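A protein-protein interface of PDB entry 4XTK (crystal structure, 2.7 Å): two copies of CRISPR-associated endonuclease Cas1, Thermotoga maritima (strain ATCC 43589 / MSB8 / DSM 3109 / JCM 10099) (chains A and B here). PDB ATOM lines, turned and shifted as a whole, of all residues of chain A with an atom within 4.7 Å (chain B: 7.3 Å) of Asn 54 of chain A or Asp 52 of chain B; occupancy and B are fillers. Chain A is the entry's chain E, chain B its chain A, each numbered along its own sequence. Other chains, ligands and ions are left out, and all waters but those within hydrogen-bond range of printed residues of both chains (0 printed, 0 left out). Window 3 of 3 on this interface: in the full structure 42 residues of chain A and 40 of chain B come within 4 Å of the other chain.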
ATOM      1  N   LEU A  19      22.639 -29.740  -3.458  1.00  0.00           N
ATOM      2  CA  LEU A  19      21.318 -30.350  -3.398  1.00  0.00           C
ATOM      3  C   LEU A  19      20.388 -29.701  -4.421  1.00  0.00           C
ATOM      4  O   LEU A  19      20.198 -28.485  -4.419  1.00  0.00           O
ATOM      5  CB  LEU A  19      20.730 -30.227  -1.992  1.00  0.00           C
ATOM      6  CG  LEU A  19      21.436 -31.031  -0.900  1.00  0.00           C
ATOM      7  CD1 LEU A  19      20.905 -30.668   0.481  1.00  0.00           C
ATOM      8  CD2 LEU A  19      21.286 -32.513  -1.159  1.00  0.00           C
ATOM      9  N   LEU A  53      22.189 -25.299  -1.699  1.00  0.00           N
ATOM     10  CA  LEU A  53      20.803 -25.512  -2.093  1.00  0.00           C
ATOM     11  C   LEU A  53      20.120 -24.170  -2.323  1.00  0.00           C
ATOM     12  O   LEU A  53      20.625 -23.129  -1.907  1.00  0.00           O
ATOM     13  CB  LEU A  53      20.051 -26.342  -1.042  1.00  0.00           C
ATOM     14  CG  LEU A  53      20.025 -25.934   0.438  1.00  0.00           C
ATOM     15  CD1 LEU A  53      18.886 -24.974   0.732  1.00  0.00           C
ATOM     16  CD2 LEU A  53      19.907 -27.165   1.327  1.00  0.00           C
ATOM     17  N   ASN A  54      18.986 -24.193  -3.012  1.00  0.00           N
ATOM     18  CA  ASN A  54      18.189 -22.987  -3.181  1.00  0.00           C
ATOM     19  C   ASN A  54      16.778 -23.162  -2.633  1.00  0.00           C
ATOM     20  O   ASN A  54      16.435 -24.219  -2.098  1.00  0.00           O
ATOM     21  CB  ASN A  54      18.142 -22.566  -4.651  1.00  0.00           C
ATOM     22  CG  ASN A  54      17.743 -23.693  -5.581  1.00  0.00           C
ATOM     23  OD1 ASN A  54      17.134 -24.680  -5.169  1.00  0.00           O
ATOM     24  ND2 ASN A  54      18.092 -23.550  -6.851  1.00  0.00           N
ATOM     25  N   LYS A  55      15.967 -22.120  -2.757  1.00  0.00           N
ATOM     26  CA  LYS A  55      14.617 -22.148  -2.218  1.00  0.00           C
ATOM     27  C   LYS A  55      13.728 -23.141  -2.970  1.00  0.00           C
ATOM     28  O   LYS A  55      12.819 -23.729  -2.386  1.00  0.00           O
ATOM     29  CB  LYS A  55      14.002 -20.750  -2.256  1.00  0.00           C
ATOM     30  CG  LYS A  55      12.665 -20.657  -1.552  1.00  0.00           C
ATOM     31  CD  LYS A  55      12.118 -19.249  -1.594  1.00  0.00           C
ATOM     32  CE  LYS A  55      11.462 -18.962  -2.927  1.00  0.00           C
ATOM     33  NZ  LYS A  55      10.914 -17.581  -2.944  1.00  0.00           N
ATOM     34  N   ARG A  56      14.001 -23.334  -4.258  1.00  0.00           N
ATOM     35  CA  ARG A  56      13.213 -24.258  -5.070  1.00  0.00           C
ATOM     36  C   ARG A  56      13.352 -25.692  -4.565  1.00  0.00           C
ATOM     37  O   ARG A  56      12.404 -26.475  -4.619  1.00  0.00           O
ATOM     38  CB  ARG A  56      13.619 -24.178  -6.542  1.00  0.00           C
ATOM     39  CG  ARG A  56      12.900 -25.191  -7.422  1.00  0.00           C
ATOM     40  CD  ARG A  56      13.411 -25.183  -8.858  1.00  0.00           C
ATOM     41  NE  ARG A  56      12.378 -24.768  -9.805  1.00  0.00           N
ATOM     42  CZ  ARG A  56      11.519 -25.598 -10.390  1.00  0.00           C
ATOM     43  NH1 ARG A  56      11.566 -26.895 -10.127  1.00  0.00           N
ATOM     44  NH2 ARG A  56      10.613 -25.130 -11.241  1.00  0.00           N
ATOM     45  N   PHE A  57      14.537 -26.027  -4.067  1.00  0.00           N
ATOM     46  CA  PHE A  57      14.774 -27.332  -3.462  1.00  0.00           C
ATOM     47  C   PHE A  57      14.016 -27.469  -2.143  1.00  0.00           C
ATOM     48  O   PHE A  57      13.455 -28.526  -1.850  1.00  0.00           O
ATOM     49  CB  PHE A  57      16.267 -27.556  -3.236  1.00  0.00           C
ATOM     50  CG  PHE A  57      16.581 -28.802  -2.461  1.00  0.00           C
ATOM     51  CD1 PHE A  57      16.584 -30.040  -3.081  1.00  0.00           C
ATOM     52  CD2 PHE A  57      16.873 -28.734  -1.109  1.00  0.00           C
ATOM     53  CE1 PHE A  57      16.875 -31.190  -2.363  1.00  0.00           C
ATOM     54  CE2 PHE A  57      17.165 -29.880  -0.389  1.00  0.00           C
ATOM     55  CZ  PHE A  57      17.166 -31.108  -1.015  1.00  0.00           C
ATOM     56  N   LEU A  58      14.012 -26.400  -1.348  1.00  0.00           N
ATOM     57  CA  LEU A  58      13.257 -26.379  -0.098  1.00  0.00           C
ATOM     58  C   LEU A  58      11.757 -26.482  -0.378  1.00  0.00           C
ATOM     59  O   LEU A  58      11.021 -27.143   0.356  1.00  0.00           O
ATOM     60  CB  LEU A  58      13.563 -25.111   0.704  1.00  0.00           C
ATOM     61  CG  LEU A  58      14.985 -24.988   1.261  1.00  0.00           C
ATOM     62  CD1 LEU A  58      15.136 -23.753   2.151  1.00  0.00           C
ATOM     63  CD2 LEU A  58      15.377 -26.248   2.012  1.00  0.00           C
ATOM     64  N   SER B  16      16.109 -11.510  -5.561  1.00  0.00           N
ATOM     65  CA  SER B  16      16.749 -12.788  -5.838  1.00  0.00           C
ATOM     66  C   SER B  16      18.271 -12.666  -5.799  1.00  0.00           C
ATOM     67  O   SER B  16      18.826 -11.636  -6.180  1.00  0.00           O
ATOM     68  CB  SER B  16      16.297 -13.319  -7.199  1.00  0.00           C
ATOM     69  OG  SER B  16      14.888 -13.460  -7.240  1.00  0.00           O
ATOM     70  N   GLY B  17      18.942 -13.717  -5.341  1.00  0.00           N
ATOM     71  CA  GLY B  17      20.390 -13.717  -5.282  1.00  0.00           C
ATOM     72  C   GLY B  17      20.984 -14.849  -4.465  1.00  0.00           C
ATOM     73  O   GLY B  17      20.357 -15.888  -4.259  1.00  0.00           O
ATOM     74  N   THR B  18      22.211 -14.642  -4.000  1.00  0.00           N
ATOM     75  CA  THR B  18      22.918 -15.647  -3.219  1.00  0.00           C
ATOM     76  C   THR B  18      23.154 -15.157  -1.796  1.00  0.00           C
ATOM     77  O   THR B  18      23.634 -14.044  -1.589  1.00  0.00           O
ATOM     78  CB  THR B  18      24.274 -16.009  -3.863  1.00  0.00           C
ATOM     79  OG1 THR B  18      24.067 -16.437  -5.215  1.00  0.00           O
ATOM     80  CG2 THR B  18      24.956 -17.121  -3.080  1.00  0.00           C
ATOM     81  N   LEU B  19      22.808 -15.989  -0.819  1.00  0.00           N
ATOM     82  CA  LEU B  19      23.026 -15.661   0.585  1.00  0.00           C
ATOM     83  C   LEU B  19      24.340 -16.228   1.100  1.00  0.00           C
ATOM     84  O   LEU B  19      24.580 -17.430   1.011  1.00  0.00           O
ATOM     85  CB  LEU B  19      21.880 -16.192   1.444  1.00  0.00           C
ATOM     86  CG  LEU B  19      20.524 -15.509   1.310  1.00  0.00           C
ATOM     87  CD1 LEU B  19      19.456 -16.343   1.994  1.00  0.00           C
ATOM     88  CD2 LEU B  19      20.588 -14.117   1.911  1.00  0.00           C
ATOM     89  N   LYS B  20      25.187 -15.359   1.643  1.00  0.00           N
ATOM     90  CA  LYS B  20      26.414 -15.796   2.297  1.00  0.00           C
ATOM     91  C   LYS B  20      26.793 -14.824   3.409  1.00  0.00           C
ATOM     92  O   LYS B  20      26.425 -13.651   3.364  1.00  0.00           O
ATOM     93  CB  LYS B  20      27.555 -15.921   1.285  1.00  0.00           C
ATOM     94  CG  LYS B  20      27.789 -14.679   0.442  1.00  0.00           C
ATOM     95  N   CYS B  27      25.185 -11.220   3.331  1.00  0.00           N
ATOM     96  CA  CYS B  27      25.261 -10.565   2.039  1.00  0.00           C
ATOM     97  C   CYS B  27      24.403 -11.280   1.013  1.00  0.00           C
ATOM     98  O   CYS B  27      24.469 -12.502   0.873  1.00  0.00           O
ATOM     99  CB  CYS B  27      26.706 -10.496   1.553  1.00  0.00           C
ATOM    100  SG  CYS B  27      26.860  -9.834  -0.107  1.00  0.00           S
ATOM    101  N   LEU B  28      23.592 -10.507   0.304  1.00  0.00           N
ATOM    102  CA  LEU B  28      22.817 -11.030  -0.807  1.00  0.00           C
ATOM    103  C   LEU B  28      23.414 -10.544  -2.118  1.00  0.00           C
ATOM    104  O   LEU B  28      23.317  -9.362  -2.442  1.00  0.00           O
ATOM    105  CB  LEU B  28      21.356 -10.599  -0.700  1.00  0.00           C
ATOM    106  CG  LEU B  28      20.417 -11.129  -1.781  1.00  0.00           C
ATOM    107  CD1 LEU B  28      20.335 -12.641  -1.697  1.00  0.00           C
ATOM    108  CD2 LEU B  28      19.039 -10.501  -1.643  1.00  0.00           C
ATOM    109  N   GLY B  49      12.071 -14.083  -2.089  1.00  0.00           N
ATOM    110  CA  GLY B  49      12.721 -14.114  -3.385  1.00  0.00           C
ATOM    111  C   GLY B  49      13.290 -15.481  -3.696  1.00  0.00           C
ATOM    112  O   GLY B  49      13.161 -16.406  -2.897  1.00  0.00           O
ATOM    113  N   GLU B  50      13.919 -15.616  -4.857  1.00  0.00           N
ATOM    114  CA  GLU B  50      14.585 -16.863  -5.202  1.00  0.00           C
ATOM    115  C   GLU B  50      16.044 -16.774  -4.776  1.00  0.00           C
ATOM    116  O   GLU B  50      16.811 -15.982  -5.318  1.00  0.00           O
ATOM    117  CB  GLU B  50      14.464 -17.154  -6.702  1.00  0.00           C
ATOM    118  CG  GLU B  50      13.022 -17.250  -7.196  1.00  0.00           C
ATOM    119  CD  GLU B  50      12.259 -18.416  -6.581  1.00  0.00           C
ATOM    120  OE1 GLU B  50      12.893 -19.437  -6.237  1.00  0.00           O
ATOM    121  OE2 GLU B  50      11.022 -18.306  -6.430  1.00  0.00           O
ATOM    122  N   VAL B  51      16.422 -17.582  -3.789  1.00  0.00           N
ATOM    123  CA  VAL B  51      17.763 -17.496  -3.224  1.00  0.00           C
ATOM    124  C   VAL B  51      18.492 -18.839  -3.182  1.00  0.00           C
ATOM    125  O   VAL B  51      17.896 -19.883  -2.903  1.00  0.00           O
ATOM    126  CB  VAL B  51      17.736 -16.906  -1.782  1.00  0.00           C
ATOM    127  CG1 VAL B  51      17.266 -15.459  -1.801  1.00  0.00           C
ATOM    128  CG2 VAL B  51      16.867 -17.750  -0.853  1.00  0.00           C
ATOM    129  N   ASP B  52      19.789 -18.790  -3.468  1.00  0.00           N
ATOM    130  CA  ASP B  52      20.687 -19.919  -3.257  1.00  0.00           C
ATOM    131  C   ASP B  52      21.462 -19.676  -1.965  1.00  0.00           C
ATOM    132  O   ASP B  52      21.765 -18.534  -1.631  1.00  0.00           O
ATOM    133  CB  ASP B  52      21.659 -20.094  -4.433  1.00  0.00           C
ATOM    134  CG  ASP B  52      20.954 -20.377  -5.755  1.00  0.00           C
ATOM    135  OD1 ASP B  52      20.738 -21.567  -6.074  1.00  0.00           O
ATOM    136  OD2 ASP B  52      20.631 -19.413  -6.484  1.00  0.00           O
ATOM    137  N   LEU B  53      21.768 -20.744  -1.235  1.00  0.00           N
ATOM    138  CA  LEU B  53      22.553 -20.637  -0.006  1.00  0.00           C
ATOM    139  C   LEU B  53      23.277 -21.949   0.296  1.00  0.00           C
ATOM    140  O   LEU B  53      22.949 -22.990  -0.268  1.00  0.00           O
ATOM    141  CB  LEU B  53      21.654 -20.234   1.168  1.00  0.00           C
ATOM    142  CG  LEU B  53      20.457 -21.133   1.492  1.00  0.00           C
ATOM    143  CD1 LEU B  53      20.839 -22.233   2.471  1.00  0.00           C
ATOM    144  CD2 LEU B  53      19.299 -20.314   2.036  1.00  0.00           C
ATOM    145  N   ASN B  54      24.267 -21.898   1.179  1.00  0.00           N
ATOM    146  CA  ASN B  54      24.951 -23.113   1.607  1.00  0.00           C
ATOM    147  C   ASN B  54      24.757 -23.375   3.098  1.00  0.00           C
ATOM    148  O   ASN B  54      24.138 -22.574   3.796  1.00  0.00           O
ATOM    149  CB  ASN B  54      26.438 -23.036   1.274  1.00  0.00           C
ATOM    150  CG  ASN B  54      27.098 -21.797   1.844  1.00  0.00           C
ATOM    151  OD1 ASN B  54      26.591 -21.180   2.778  1.00  0.00           O
ATOM    152  ND2 ASN B  54      28.238 -21.425   1.277  1.00  0.00           N
ATOM    153  N   PHE B  57      26.233 -20.837   5.609  1.00  0.00           N
ATOM    154  CA  PHE B  57      25.347 -19.712   5.863  1.00  0.00           C
ATOM    155  C   PHE B  57      24.361 -20.034   6.977  1.00  0.00           C
ATOM    156  O   PHE B  57      24.047 -19.177   7.801  1.00  0.00           O
ATOM    157  CB  PHE B  57      24.587 -19.313   4.599  1.00  0.00           C
ATOM    158  CG  PHE B  57      23.561 -18.247   4.837  1.00  0.00           C
ATOM    159  CD1 PHE B  57      23.952 -16.933   5.039  1.00  0.00           C
ATOM    160  CD2 PHE B  57      22.210 -18.556   4.873  1.00  0.00           C
ATOM    161  CE1 PHE B  57      23.016 -15.947   5.267  1.00  0.00           C
ATOM    162  CE2 PHE B  57      21.264 -17.570   5.099  1.00  0.00           C
ATOM    163  CZ  PHE B  57      21.669 -16.265   5.297  1.00  0.00           C
ATOM    164  N   PHE B  70      10.848 -19.165   4.838  1.00  0.00           N
ATOM    165  CA  PHE B  70      10.809 -19.157   3.386  1.00  0.00           C
ATOM    166  C   PHE B  70       9.377 -19.119   2.873  1.00  0.00           C
ATOM    167  O   PHE B  70       8.500 -19.831   3.369  1.00  0.00           O
ATOM    168  CB  PHE B  70      11.551 -20.376   2.828  1.00  0.00           C
ATOM    169  CG  PHE B  70      13.020 -20.367   3.119  1.00  0.00           C
ATOM    170  CD1 PHE B  70      13.900 -19.702   2.280  1.00  0.00           C
ATOM    171  CD2 PHE B  70      13.521 -20.999   4.251  1.00  0.00           C
ATOM    172  CE1 PHE B  70      15.256 -19.683   2.552  1.00  0.00           C
ATOM    173  CE2 PHE B  70      14.876 -20.982   4.529  1.00  0.00           C
ATOM    174  CZ  PHE B  70      15.744 -20.324   3.678  1.00  0.00           C
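O of Gly 49 of chain B is in hydrogen-bond range of NZ of Lys 55 of chain A, at 2.5 Å.
OE2 of Glu 50 of chain B lies within salt-bridge range of NZ of Lys 55 of chain A.
The backbone NH (N) of Leu 53 of chain B is in hydrogen-bond range of the backbone carbonyl oxygen (O) of Leu 53 of chain A, 2.7 Å away.
The backbone carbonyl oxygen of Val 51 of chain B sits at hydrogen-bond distance from the backbone NH of Lys 55 of chain A.
OD1 of Asp 52 of chain B sits close to ND2 of Asn 54 of chain A (3.4 Å).
The side-chain amide oxygen (OD1) of Asn 54 of chain A is in hydrogen-bond range of the backbone NH (N) of Phe 57 of chain A, 3.1 Å away.
The backbone carbonyl oxygen (O) of Asp 52 of chain B sits at hydrogen-bond distance from the backbone NH (N) of Leu 19 of chain B (2.9 Å).
OG of Ser 16 of chain B lies within hydrogen-bond range of N of Glu 50 of chain B (3.4 Å).
The backbone carbonyl oxygen (O) of Gly 17 of chain B sits at hydrogen-bond distance from the backbone NH (N) of Asp 52 of chain B (3.1 Å).
The backbone NH (N) of Gly 17 of chain B lies within hydrogen-bond range of the backbone carbonyl oxygen (O) of Glu 50 of chain B, at 3.1 Å.
Among the printed residues, pairs that only touch across the chains: Leu 53 of chain A with Asp 52 of chain B (3.5 Å), Asn 54 of chain A with Val 51 of chain B (3.1 Å) and Leu 58 of chain A with Phe 70 of chain B (3.7 Å).
Asn 54 of chain A touches just these residues of chain B: Val 51 and Asp 52.
Printed residues of chain B within 4 Å of Leu 58 of chain A: Phe 70 (3.7 Å).
Ser 16 of chain B touches none of the printed residues of chain A.
Of the printed residues of chain A, Gly 49 of chain B touches Lys 55.
The nearest residue of chain B that does not touch Asn 54 of chain A is Leu 53 of chain B (4.7 Å).
The nearest printed residue of chain A that does not touch Asp 52 of chain B is Lys 55 of chain A (5.1 Å).
The nearest printed residue of chain A that does not touch Leu 53 of chain B is Asn 54 of chain A (4.7 Å).
Of the 15 printed residues of chain B, 6 touch a printed residue of chain A.
Hydrophobic or aromatic side chains of chain B within 4 Å of the printed part of chain A: Leu 53 and Phe 70.
Of the 7 printed residues of chain A, 4 touch a printed residue of chain B.
Printed residues of chain A that touch a printed residue of chain B: Leu 53, Asn 54, Lys 55 and Leu 58.
Among the printed residues, Asp or Glu carboxylates within 4 Å of a Lys or Arg side-chain nitrogen of the other chain: Lys 55 of chain A with Glu 50 of chain B.
Leu 53 of chain B touches its own counterpart, Leu 53 of chain A.
Of the 8 pairs that touch across the chains among the printed residues, 1 has its exchanged pair printed and touching as well.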
